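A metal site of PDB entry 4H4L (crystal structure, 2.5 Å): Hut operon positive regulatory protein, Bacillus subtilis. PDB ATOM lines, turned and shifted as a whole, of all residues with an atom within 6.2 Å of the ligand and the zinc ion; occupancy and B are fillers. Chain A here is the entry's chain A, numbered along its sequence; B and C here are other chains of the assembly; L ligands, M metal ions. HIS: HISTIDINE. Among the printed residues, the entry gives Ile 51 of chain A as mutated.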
ATOM      1  N   ILE A  51      25.673  -9.783 -12.577  1.00  0.00           N
ATOM      2  CA  ILE A  51      25.759 -10.793 -13.619  1.00  0.00           C
ATOM      3  C   ILE A  51      25.232 -10.241 -14.966  1.00  0.00           C
ATOM      4  O   ILE A  51      25.861 -10.445 -16.011  1.00  0.00           O
ATOM      5  CB  ILE A  51      25.000 -12.087 -13.172  1.00  0.00           C
ATOM      6  CG1 ILE A  51      25.631 -12.642 -11.897  1.00  0.00           C
ATOM      7  CG2 ILE A  51      24.925 -13.125 -14.289  1.00  0.00           C
ATOM      8  CD1 ILE A  51      24.781 -13.675 -11.194  1.00  0.00           C
ATOM      9  N   GLU A  55      26.876  -9.597 -18.600  1.00  0.00           N
ATOM     10  CA  GLU A  55      26.454 -10.411 -19.734  1.00  0.00           C
ATOM     11  C   GLU A  55      26.226  -9.467 -20.902  1.00  0.00           C
ATOM     12  O   GLU A  55      26.765  -9.668 -22.015  1.00  0.00           O
ATOM     13  CB  GLU A  55      25.183 -11.172 -19.422  1.00  0.00           C
ATOM     14  CG  GLU A  55      24.789 -12.243 -20.431  1.00  0.00           C
ATOM     15  CD  GLU A  55      23.394 -12.829 -20.185  1.00  0.00           C
ATOM     16  OE1 GLU A  55      22.702 -12.432 -19.210  1.00  0.00           O
ATOM     17  OE2 GLU A  55      22.954 -13.676 -20.971  1.00  0.00           O
ATOM     18  N   TYR A  69      23.644 -20.683 -26.499  1.00  0.00           N
ATOM     19  CA  TYR A  69      23.868 -20.896 -25.076  1.00  0.00           C
ATOM     20  C   TYR A  69      25.350 -21.050 -24.713  1.00  0.00           C
ATOM     21  O   TYR A  69      25.859 -20.414 -23.785  1.00  0.00           O
ATOM     22  CB  TYR A  69      23.093 -22.132 -24.630  1.00  0.00           C
ATOM     23  CG  TYR A  69      22.981 -22.314 -23.124  1.00  0.00           C
ATOM     24  CD1 TYR A  69      22.795 -21.201 -22.281  1.00  0.00           C
ATOM     25  CD2 TYR A  69      23.024 -23.578 -22.544  1.00  0.00           C
ATOM     26  CE1 TYR A  69      22.675 -21.361 -20.921  1.00  0.00           C
ATOM     27  CE2 TYR A  69      22.898 -23.741 -21.176  1.00  0.00           C
ATOM     28  CZ  TYR A  69      22.733 -22.620 -20.379  1.00  0.00           C
ATOM     29  OH  TYR A  69      22.611 -22.741 -19.030  1.00  0.00           O
ATOM     30  N   SER A  72      27.373 -18.221 -23.377  1.00  0.00           N
ATOM     31  CA  SER A  72      26.746 -17.638 -22.197  1.00  0.00           C
ATOM     32  C   SER A  72      26.978 -18.490 -20.982  1.00  0.00           C
ATOM     33  O   SER A  72      27.257 -17.960 -19.916  1.00  0.00           O
ATOM     34  CB  SER A  72      25.254 -17.464 -22.411  1.00  0.00           C
ATOM     35  OG  SER A  72      25.060 -16.421 -23.312  1.00  0.00           O
ATOM     36  N   HIS A  73      26.857 -19.803 -21.139  1.00  0.00           N
ATOM     37  CA  HIS A  73      27.131 -20.721 -20.044  1.00  0.00           C
ATOM     38  C   HIS A  73      28.533 -20.588 -19.470  1.00  0.00           C
ATOM     39  O   HIS A  73      28.730 -20.718 -18.269  1.00  0.00           O
ATOM     40  CB  HIS A  73      26.876 -22.138 -20.482  1.00  0.00           C
ATOM     41  CG  HIS A  73      26.928 -23.128 -19.355  1.00  0.00           C
ATOM     42  ND1 HIS A  73      28.070 -23.697 -18.959  1.00  0.00           N
ATOM     43  CD2 HIS A  73      25.924 -23.662 -18.560  1.00  0.00           C
ATOM     44  CE1 HIS A  73      27.820 -24.552 -17.962  1.00  0.00           C
ATOM     45  NE2 HIS A  73      26.503 -24.529 -17.712  1.00  0.00           N
ATOM     46  N   TYR A  76      28.454 -17.228 -17.743  1.00  0.00           N
ATOM     47  CA  TYR A  76      27.651 -17.263 -16.559  1.00  0.00           C
ATOM     48  C   TYR A  76      28.538 -17.814 -15.465  1.00  0.00           C
ATOM     49  O   TYR A  76      28.768 -17.167 -14.426  1.00  0.00           O
ATOM     50  CB  TYR A  76      26.412 -18.100 -16.710  1.00  0.00           C
ATOM     51  CG  TYR A  76      25.604 -18.114 -15.436  1.00  0.00           C
ATOM     52  CD1 TYR A  76      24.872 -16.973 -15.027  1.00  0.00           C
ATOM     53  CD2 TYR A  76      25.587 -19.254 -14.627  1.00  0.00           C
ATOM     54  CE1 TYR A  76      24.157 -17.000 -13.822  1.00  0.00           C
ATOM     55  CE2 TYR A  76      24.872 -19.289 -13.449  1.00  0.00           C
ATOM     56  CZ  TYR A  76      24.167 -18.169 -13.055  1.00  0.00           C
ATOM     57  OH  TYR A  76      23.482 -18.245 -11.873  1.00  0.00           O
ATOM     58  N   HIS A  77      29.136 -18.965 -15.741  1.00  0.00           N
ATOM     59  CA  HIS A  77      29.917 -19.640 -14.746  1.00  0.00           C
ATOM     60  C   HIS A  77      31.173 -18.965 -14.358  1.00  0.00           C
ATOM     61  O   HIS A  77      31.566 -19.049 -13.189  1.00  0.00           O
ATOM     62  CB  HIS A  77      30.152 -21.072 -15.153  1.00  0.00           C
ATOM     63  CG  HIS A  77      28.935 -21.938 -14.942  1.00  0.00           C
ATOM     64  ND1 HIS A  77      28.602 -22.409 -13.739  1.00  0.00           N
ATOM     65  CD2 HIS A  77      27.969 -22.371 -15.816  1.00  0.00           C
ATOM     66  CE1 HIS A  77      27.472 -23.117 -13.838  1.00  0.00           C
ATOM     67  NE2 HIS A  77      27.089 -23.113 -15.115  1.00  0.00           N
ATOM     68  N   ARG B  88      23.476 -26.635  -6.841  1.00  0.00           N
ATOM     69  CA  ARG B  88      24.890 -26.861  -6.929  1.00  0.00           C
ATOM     70  C   ARG B  88      25.798 -25.793  -6.326  1.00  0.00           C
ATOM     71  O   ARG B  88      26.816 -25.445  -6.905  1.00  0.00           O
ATOM     72  CB  ARG B  88      25.289 -27.108  -8.406  1.00  0.00           C
ATOM     73  CG  ARG B  88      24.925 -28.511  -8.908  1.00  0.00           C
ATOM     74  CD  ARG B  88      24.419 -28.503 -10.335  1.00  0.00           C
ATOM     75  NE  ARG B  88      23.380 -27.479 -10.543  1.00  0.00           N
ATOM     76  CZ  ARG B  88      23.503 -26.415 -11.336  1.00  0.00           C
ATOM     77  NH1 ARG B  88      24.633 -26.198 -12.003  1.00  0.00           N
ATOM     78  NH2 ARG B  88      22.481 -25.582 -11.453  1.00  0.00           N
ATOM     79  N   LEU B  96      20.524 -14.873  -8.367  1.00  0.00           N
ATOM     80  CA  LEU B  96      21.716 -15.115  -9.218  1.00  0.00           C
ATOM     81  C   LEU B  96      21.360 -15.209 -10.673  1.00  0.00           C
ATOM     82  O   LEU B  96      22.099 -15.817 -11.432  1.00  0.00           O
ATOM     83  CB  LEU B  96      22.493 -16.366  -8.823  1.00  0.00           C
ATOM     84  CG  LEU B  96      23.173 -16.446  -7.448  1.00  0.00           C
ATOM     85  CD1 LEU B  96      23.779 -17.837  -7.273  1.00  0.00           C
ATOM     86  CD2 LEU B  96      24.238 -15.351  -7.254  1.00  0.00           C
ATOM     87  N   LEU B  97      20.213 -14.643 -11.060  1.00  0.00           N
ATOM     88  CA  LEU B  97      19.835 -14.481 -12.463  1.00  0.00           C
ATOM     89  C   LEU B  97      19.677 -15.799 -13.201  1.00  0.00           C
ATOM     90  O   LEU B  97      20.190 -15.952 -14.313  1.00  0.00           O
ATOM     91  CB  LEU B  97      20.837 -13.602 -13.224  1.00  0.00           C
ATOM     92  CG  LEU B  97      20.211 -12.959 -14.465  1.00  0.00           C
ATOM     93  CD1 LEU B  97      19.313 -11.752 -14.150  1.00  0.00           C
ATOM     94  CD2 LEU B  97      21.311 -12.592 -15.468  1.00  0.00           C
ATOM     95  N   ARG B  98      18.984 -16.733 -12.561  1.00  0.00           N
ATOM     96  CA  ARG B  98      18.658 -18.002 -13.189  1.00  0.00           C
ATOM     97  C   ARG B  98      17.297 -18.461 -12.729  1.00  0.00           C
ATOM     98  O   ARG B  98      16.768 -17.948 -11.734  1.00  0.00           O
ATOM     99  CB  ARG B  98      19.730 -19.074 -12.916  1.00  0.00           C
ATOM    100  CG  ARG B  98      19.686 -19.707 -11.538  1.00  0.00           C
ATOM    101  CD  ARG B  98      20.975 -20.464 -11.300  1.00  0.00           C
ATOM    102  NE  ARG B  98      21.096 -20.771  -9.889  1.00  0.00           N
ATOM    103  CZ  ARG B  98      22.012 -21.540  -9.336  1.00  0.00           C
ATOM    104  NH1 ARG B  98      22.925 -22.166 -10.066  1.00  0.00           N
ATOM    105  NH2 ARG B  98      21.977 -21.699  -8.019  1.00  0.00           N
ATOM    106  N   THR B  99      16.723 -19.415 -13.464  1.00  0.00           N
ATOM    107  CA  THR B  99      15.339 -19.822 -13.247  1.00  0.00           C
ATOM    108  C   THR B  99      15.198 -21.319 -13.507  1.00  0.00           C
ATOM    109  O   THR B  99      16.068 -21.916 -14.143  1.00  0.00           O
ATOM    110  CB  THR B  99      14.343 -18.937 -14.069  1.00  0.00           C
ATOM    111  OG1 THR B  99      12.987 -19.364 -13.816  1.00  0.00           O
ATOM    112  CG2 THR B  99      14.649 -19.008 -15.567  1.00  0.00           C
ATOM    113  N   ILE B 129      17.386 -25.619 -15.839  1.00  0.00           N
ATOM    114  CA  ILE B 129      17.817 -24.437 -15.126  1.00  0.00           C
ATOM    115  C   ILE B 129      18.606 -23.627 -16.119  1.00  0.00           C
ATOM    116  O   ILE B 129      19.378 -24.193 -16.905  1.00  0.00           O
ATOM    117  CB  ILE B 129      18.632 -24.755 -13.835  1.00  0.00           C
ATOM    118  CG1 ILE B 129      18.886 -23.473 -13.013  1.00  0.00           C
ATOM    119  CG2 ILE B 129      19.929 -25.529 -14.129  1.00  0.00           C
ATOM    120  CD1 ILE B 129      19.707 -23.729 -11.784  1.00  0.00           C
ATOM    121  N   GLY B 130      18.383 -22.322 -16.133  1.00  0.00           N
ATOM    122  CA  GLY B 130      19.098 -21.476 -17.048  1.00  0.00           C
ATOM    123  C   GLY B 130      18.763 -20.041 -16.828  1.00  0.00           C
ATOM    124  O   GLY B 130      18.108 -19.684 -15.820  1.00  0.00           O
ATOM    125  N   ALA B 131      19.178 -19.232 -17.811  1.00  0.00           N
ATOM    126  CA  ALA B 131      18.908 -17.791 -17.893  1.00  0.00           C
ATOM    127  C   ALA B 131      17.420 -17.541 -18.113  1.00  0.00           C
ATOM    128  O   ALA B 131      16.699 -18.455 -18.545  1.00  0.00           O
ATOM    129  CB  ALA B 131      19.719 -17.187 -19.018  1.00  0.00           C
ATOM    130  N   PRO B 132      16.940 -16.315 -17.798  1.00  0.00           N
ATOM    131  CA  PRO B 132      15.513 -16.057 -18.102  1.00  0.00           C
ATOM    132  C   PRO B 132      15.135 -16.099 -19.601  1.00  0.00           C
ATOM    133  O   PRO B 132      14.005 -16.418 -19.921  1.00  0.00           O
ATOM    134  CB  PRO B 132      15.248 -14.683 -17.488  1.00  0.00           C
ATOM    135  CG  PRO B 132      16.588 -14.127 -17.101  1.00  0.00           C
ATOM    136  CD  PRO B 132      17.521 -15.269 -16.927  1.00  0.00           C
ATOM    137  N   LEU B 136      17.922 -20.877 -23.107  1.00  0.00           N
ATOM    138  CA  LEU B 136      19.283 -20.764 -22.652  1.00  0.00           C
ATOM    139  C   LEU B 136      19.378 -21.499 -21.310  1.00  0.00           C
ATOM    140  O   LEU B 136      19.298 -20.859 -20.258  1.00  0.00           O
ATOM    141  CB  LEU B 136      19.687 -19.287 -22.531  1.00  0.00           C
ATOM    142  CG  LEU B 136      19.556 -18.375 -23.747  1.00  0.00           C
ATOM    143  CD1 LEU B 136      20.573 -17.260 -23.663  1.00  0.00           C
ATOM    144  CD2 LEU B 136      19.760 -19.149 -25.039  1.00  0.00           C
ATOM    145  N   GLU B 137      19.555 -22.825 -21.357  1.00  0.00           N
ATOM    146  CA  GLU B 137      19.435 -23.680 -20.167  1.00  0.00           C
ATOM    147  C   GLU B 137      20.039 -25.069 -20.376  1.00  0.00           C
ATOM    148  O   GLU B 137      20.213 -25.519 -21.510  1.00  0.00           O
ATOM    149  CB  GLU B 137      17.957 -23.827 -19.782  1.00  0.00           C
ATOM    150  CG  GLU B 137      17.145 -24.660 -20.761  1.00  0.00           C
ATOM    151  CD  GLU B 137      15.738 -24.144 -20.961  1.00  0.00           C
ATOM    152  OE1 GLU B 137      15.556 -22.910 -20.961  1.00  0.00           O
ATOM    153  OE2 GLU B 137      14.810 -24.958 -21.130  1.00  0.00           O
ATOM    154  N   HIS B 138      20.388 -25.729 -19.265  1.00  0.00           N
ATOM    155  CA  HIS B 138      20.641 -27.156 -19.275  1.00  0.00           C
ATOM    156  C   HIS B 138      19.715 -27.806 -18.300  1.00  0.00           C
ATOM    157  O   HIS B 138      18.979 -27.112 -17.557  1.00  0.00           O
ATOM    158  CB  HIS B 138      22.106 -27.547 -19.007  1.00  0.00           C
ATOM    159  CG  HIS B 138      22.730 -26.905 -17.771  1.00  0.00           C
ATOM    160  ND1 HIS B 138      22.358 -27.235 -16.505  1.00  0.00           N
ATOM    161  CD2 HIS B 138      23.726 -26.015 -17.630  1.00  0.00           C
ATOM    162  CE1 HIS B 138      23.089 -26.501 -15.625  1.00  0.00           C
ATOM    163  NE2 HIS B 138      23.936 -25.734 -16.326  1.00  0.00           N
ATOM    164  N   GLU C  81      30.023 -30.480  -9.620  1.00  0.00           N
ATOM    165  CA  GLU C  81      28.632 -30.136  -9.660  1.00  0.00           C
ATOM    166  C   GLU C  81      27.795 -31.318  -9.260  1.00  0.00           C
ATOM    167  O   GLU C  81      26.853 -31.186  -8.463  1.00  0.00           O
ATOM    168  CB  GLU C  81      28.245 -29.630 -11.058  1.00  0.00           C
ATOM    169  CG  GLU C  81      28.621 -28.165 -11.279  1.00  0.00           C
ATOM    170  CD  GLU C  81      27.735 -27.458 -12.292  1.00  0.00           C
ATOM    171  OE1 GLU C  81      28.119 -26.335 -12.702  1.00  0.00           O
ATOM    172  OE2 GLU C  81      26.662 -27.998 -12.665  1.00  0.00           O
ATOM    173  N   TRP C 120      28.478 -31.435 -25.231  1.00  0.00           N
ATOM    174  CA  TRP C 120      28.203 -31.208 -23.806  1.00  0.00           C
ATOM    175  C   TRP C 120      28.385 -32.447 -22.982  1.00  0.00           C
ATOM    176  O   TRP C 120      28.040 -33.553 -23.392  1.00  0.00           O
ATOM    177  CB  TRP C 120      26.798 -30.687 -23.596  1.00  0.00           C
ATOM    178  CG  TRP C 120      26.645 -29.233 -23.945  1.00  0.00           C
ATOM    179  CD1 TRP C 120      26.678 -28.652 -25.212  1.00  0.00           C
ATOM    180  CD2 TRP C 120      26.409 -28.119 -23.022  1.00  0.00           C
ATOM    181  NE1 TRP C 120      26.491 -27.298 -25.136  1.00  0.00           N
ATOM    182  CE2 TRP C 120      26.321 -26.916 -23.850  1.00  0.00           C
ATOM    183  CE3 TRP C 120      26.256 -28.001 -21.646  1.00  0.00           C
ATOM    184  CZ2 TRP C 120      26.097 -25.666 -23.304  1.00  0.00           C
ATOM    185  CZ3 TRP C 120      26.030 -26.741 -21.110  1.00  0.00           C
ATOM    186  CH2 TRP C 120      25.954 -25.608 -21.918  1.00  0.00           C
ATOM    187  N   ILE C 145      26.364 -30.836 -15.273  1.00  0.00           N
ATOM    188  CA  ILE C 145      26.309 -30.582 -16.699  1.00  0.00           C
ATOM    189  C   ILE C 145      27.151 -29.385 -17.066  1.00  0.00           C
ATOM    190  O   ILE C 145      26.981 -28.319 -16.489  1.00  0.00           O
ATOM    191  CB  ILE C 145      24.852 -30.455 -17.142  1.00  0.00           C
ATOM    192  CG1 ILE C 145      24.296 -31.864 -17.299  1.00  0.00           C
ATOM    193  CG2 ILE C 145      24.754 -29.735 -18.479  1.00  0.00           C
ATOM    194  CD1 ILE C 145      22.811 -31.979 -17.276  1.00  0.00           C
ATOM    195  N   ASN C 146      28.081 -29.585 -18.005  1.00  0.00           N
ATOM    196  CA  ASN C 146      28.958 -28.525 -18.510  1.00  0.00           C
ATOM    197  C   ASN C 146      29.111 -28.595 -20.017  1.00  0.00           C
ATOM    198  O   ASN C 146      28.843 -29.641 -20.642  1.00  0.00           O
ATOM    199  CB  ASN C 146      30.336 -28.666 -17.888  1.00  0.00           C
ATOM    200  CG  ASN C 146      31.036 -27.303 -17.694  1.00  0.00           C
ATOM    201  OD1 ASN C 146      30.486 -26.245 -18.001  1.00  0.00           O
ATOM    202  ND2 ASN C 146      32.247 -27.339 -17.177  1.00  0.00           N
HETATM  203  N   HIS L   1      21.451 -17.953 -15.457  1.00  0.00           N
HETATM  204  CA  HIS L   1      22.317 -19.146 -15.615  1.00  0.00           C
HETATM  205  C   HIS L   1      22.596 -19.327 -17.045  1.00  0.00           C
HETATM  206  O   HIS L   1      23.084 -18.377 -17.611  1.00  0.00           O
HETATM  207  CB  HIS L   1      21.683 -20.422 -15.046  1.00  0.00           C
HETATM  208  CG  HIS L   1      22.651 -21.577 -14.942  1.00  0.00           C
HETATM  209  ND1 HIS L   1      22.768 -22.355 -13.822  1.00  0.00           N
HETATM  210  CD2 HIS L   1      23.596 -22.039 -15.829  1.00  0.00           C
HETATM  211  CE1 HIS L   1      23.712 -23.275 -14.020  1.00  0.00           C
HETATM  212  NE2 HIS L   1      24.222 -23.068 -15.242  1.00  0.00           N
HETATM  213  OXT HIS L   1      22.351 -20.396 -17.626  1.00  0.00           O
HETATM  214 ZN    ZN M   1      25.582 -24.504 -15.766  1.00  0.00          ZN
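An oxygen (OXT) of the ligand lies within hydrogen-bond range of the backbone NH (N) of Ala 131 of chain B (3.4 Å). The backbone carbonyl oxygen of Leu 97 of chain B sits at hydrogen-bond distance from a nitrogen (N) of the ligand (2.6 Å). OH of Tyr 69 is in hydrogen-bond range of OXT of the ligand (2.7 Å).
The backbone NH of Ile 129 of chain B sits at hydrogen-bond distance from the backbone carbonyl oxygen of His 138 of chain B, at 2.8 Å. The side-chain carboxylate of Glu 81 of chain C lies within salt-bridge range of the guanidinium group of Arg 88 of chain B, at 2.8 Å. N of Ala 131 of chain B sits at hydrogen-bond distance from O of Leu 136 of chain B, at 2.9 Å. The backbone carbonyl oxygen of Gly 130 of chain B sits at hydrogen-bond distance from the backbone NH of Thr 99 of chain B (2.7 Å). O of Leu 96 of chain B lies within hydrogen-bond range of OH of Tyr 76 (2.8 Å).
Residues that only touch the ligand: Arg 98 of chain B, Tyr 76, Gly 130 of chain B, Arg 88 of chain B and Ile 129 of chain B. Hydrophobic or aromatic side chains within 4 Å of the ligand: Tyr 69, His 73, Tyr 76, His 77, Ile 129 of chain B, Ala 131 of chain B and His 138 of chain B. Of the 23 residues printed, 11 come within 4 Å of the ligand. Along chain A the residues within 4 Å of the ligand span positions 69 to 77.
Within 4 Å of the zinc ion: His 73, His 77 and His 138 of chain B. Along chain A the residues within 4 Å of the zinc ion span positions 73 to 77. The nearest printed residue that does not touch the zinc ion is Ile 145 of chain C (4.1 Å).
NE2 of the ligand binds the zinc ion, 2.0 Å away. A ring nitrogen (NE2) of His 138 of chain B binds the zinc ion (2.1 Å). A ring nitrogen (NE2) of His 77 binds the zinc ion. NE2 of His 73 binds the zinc ion, at 2.2 Å.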
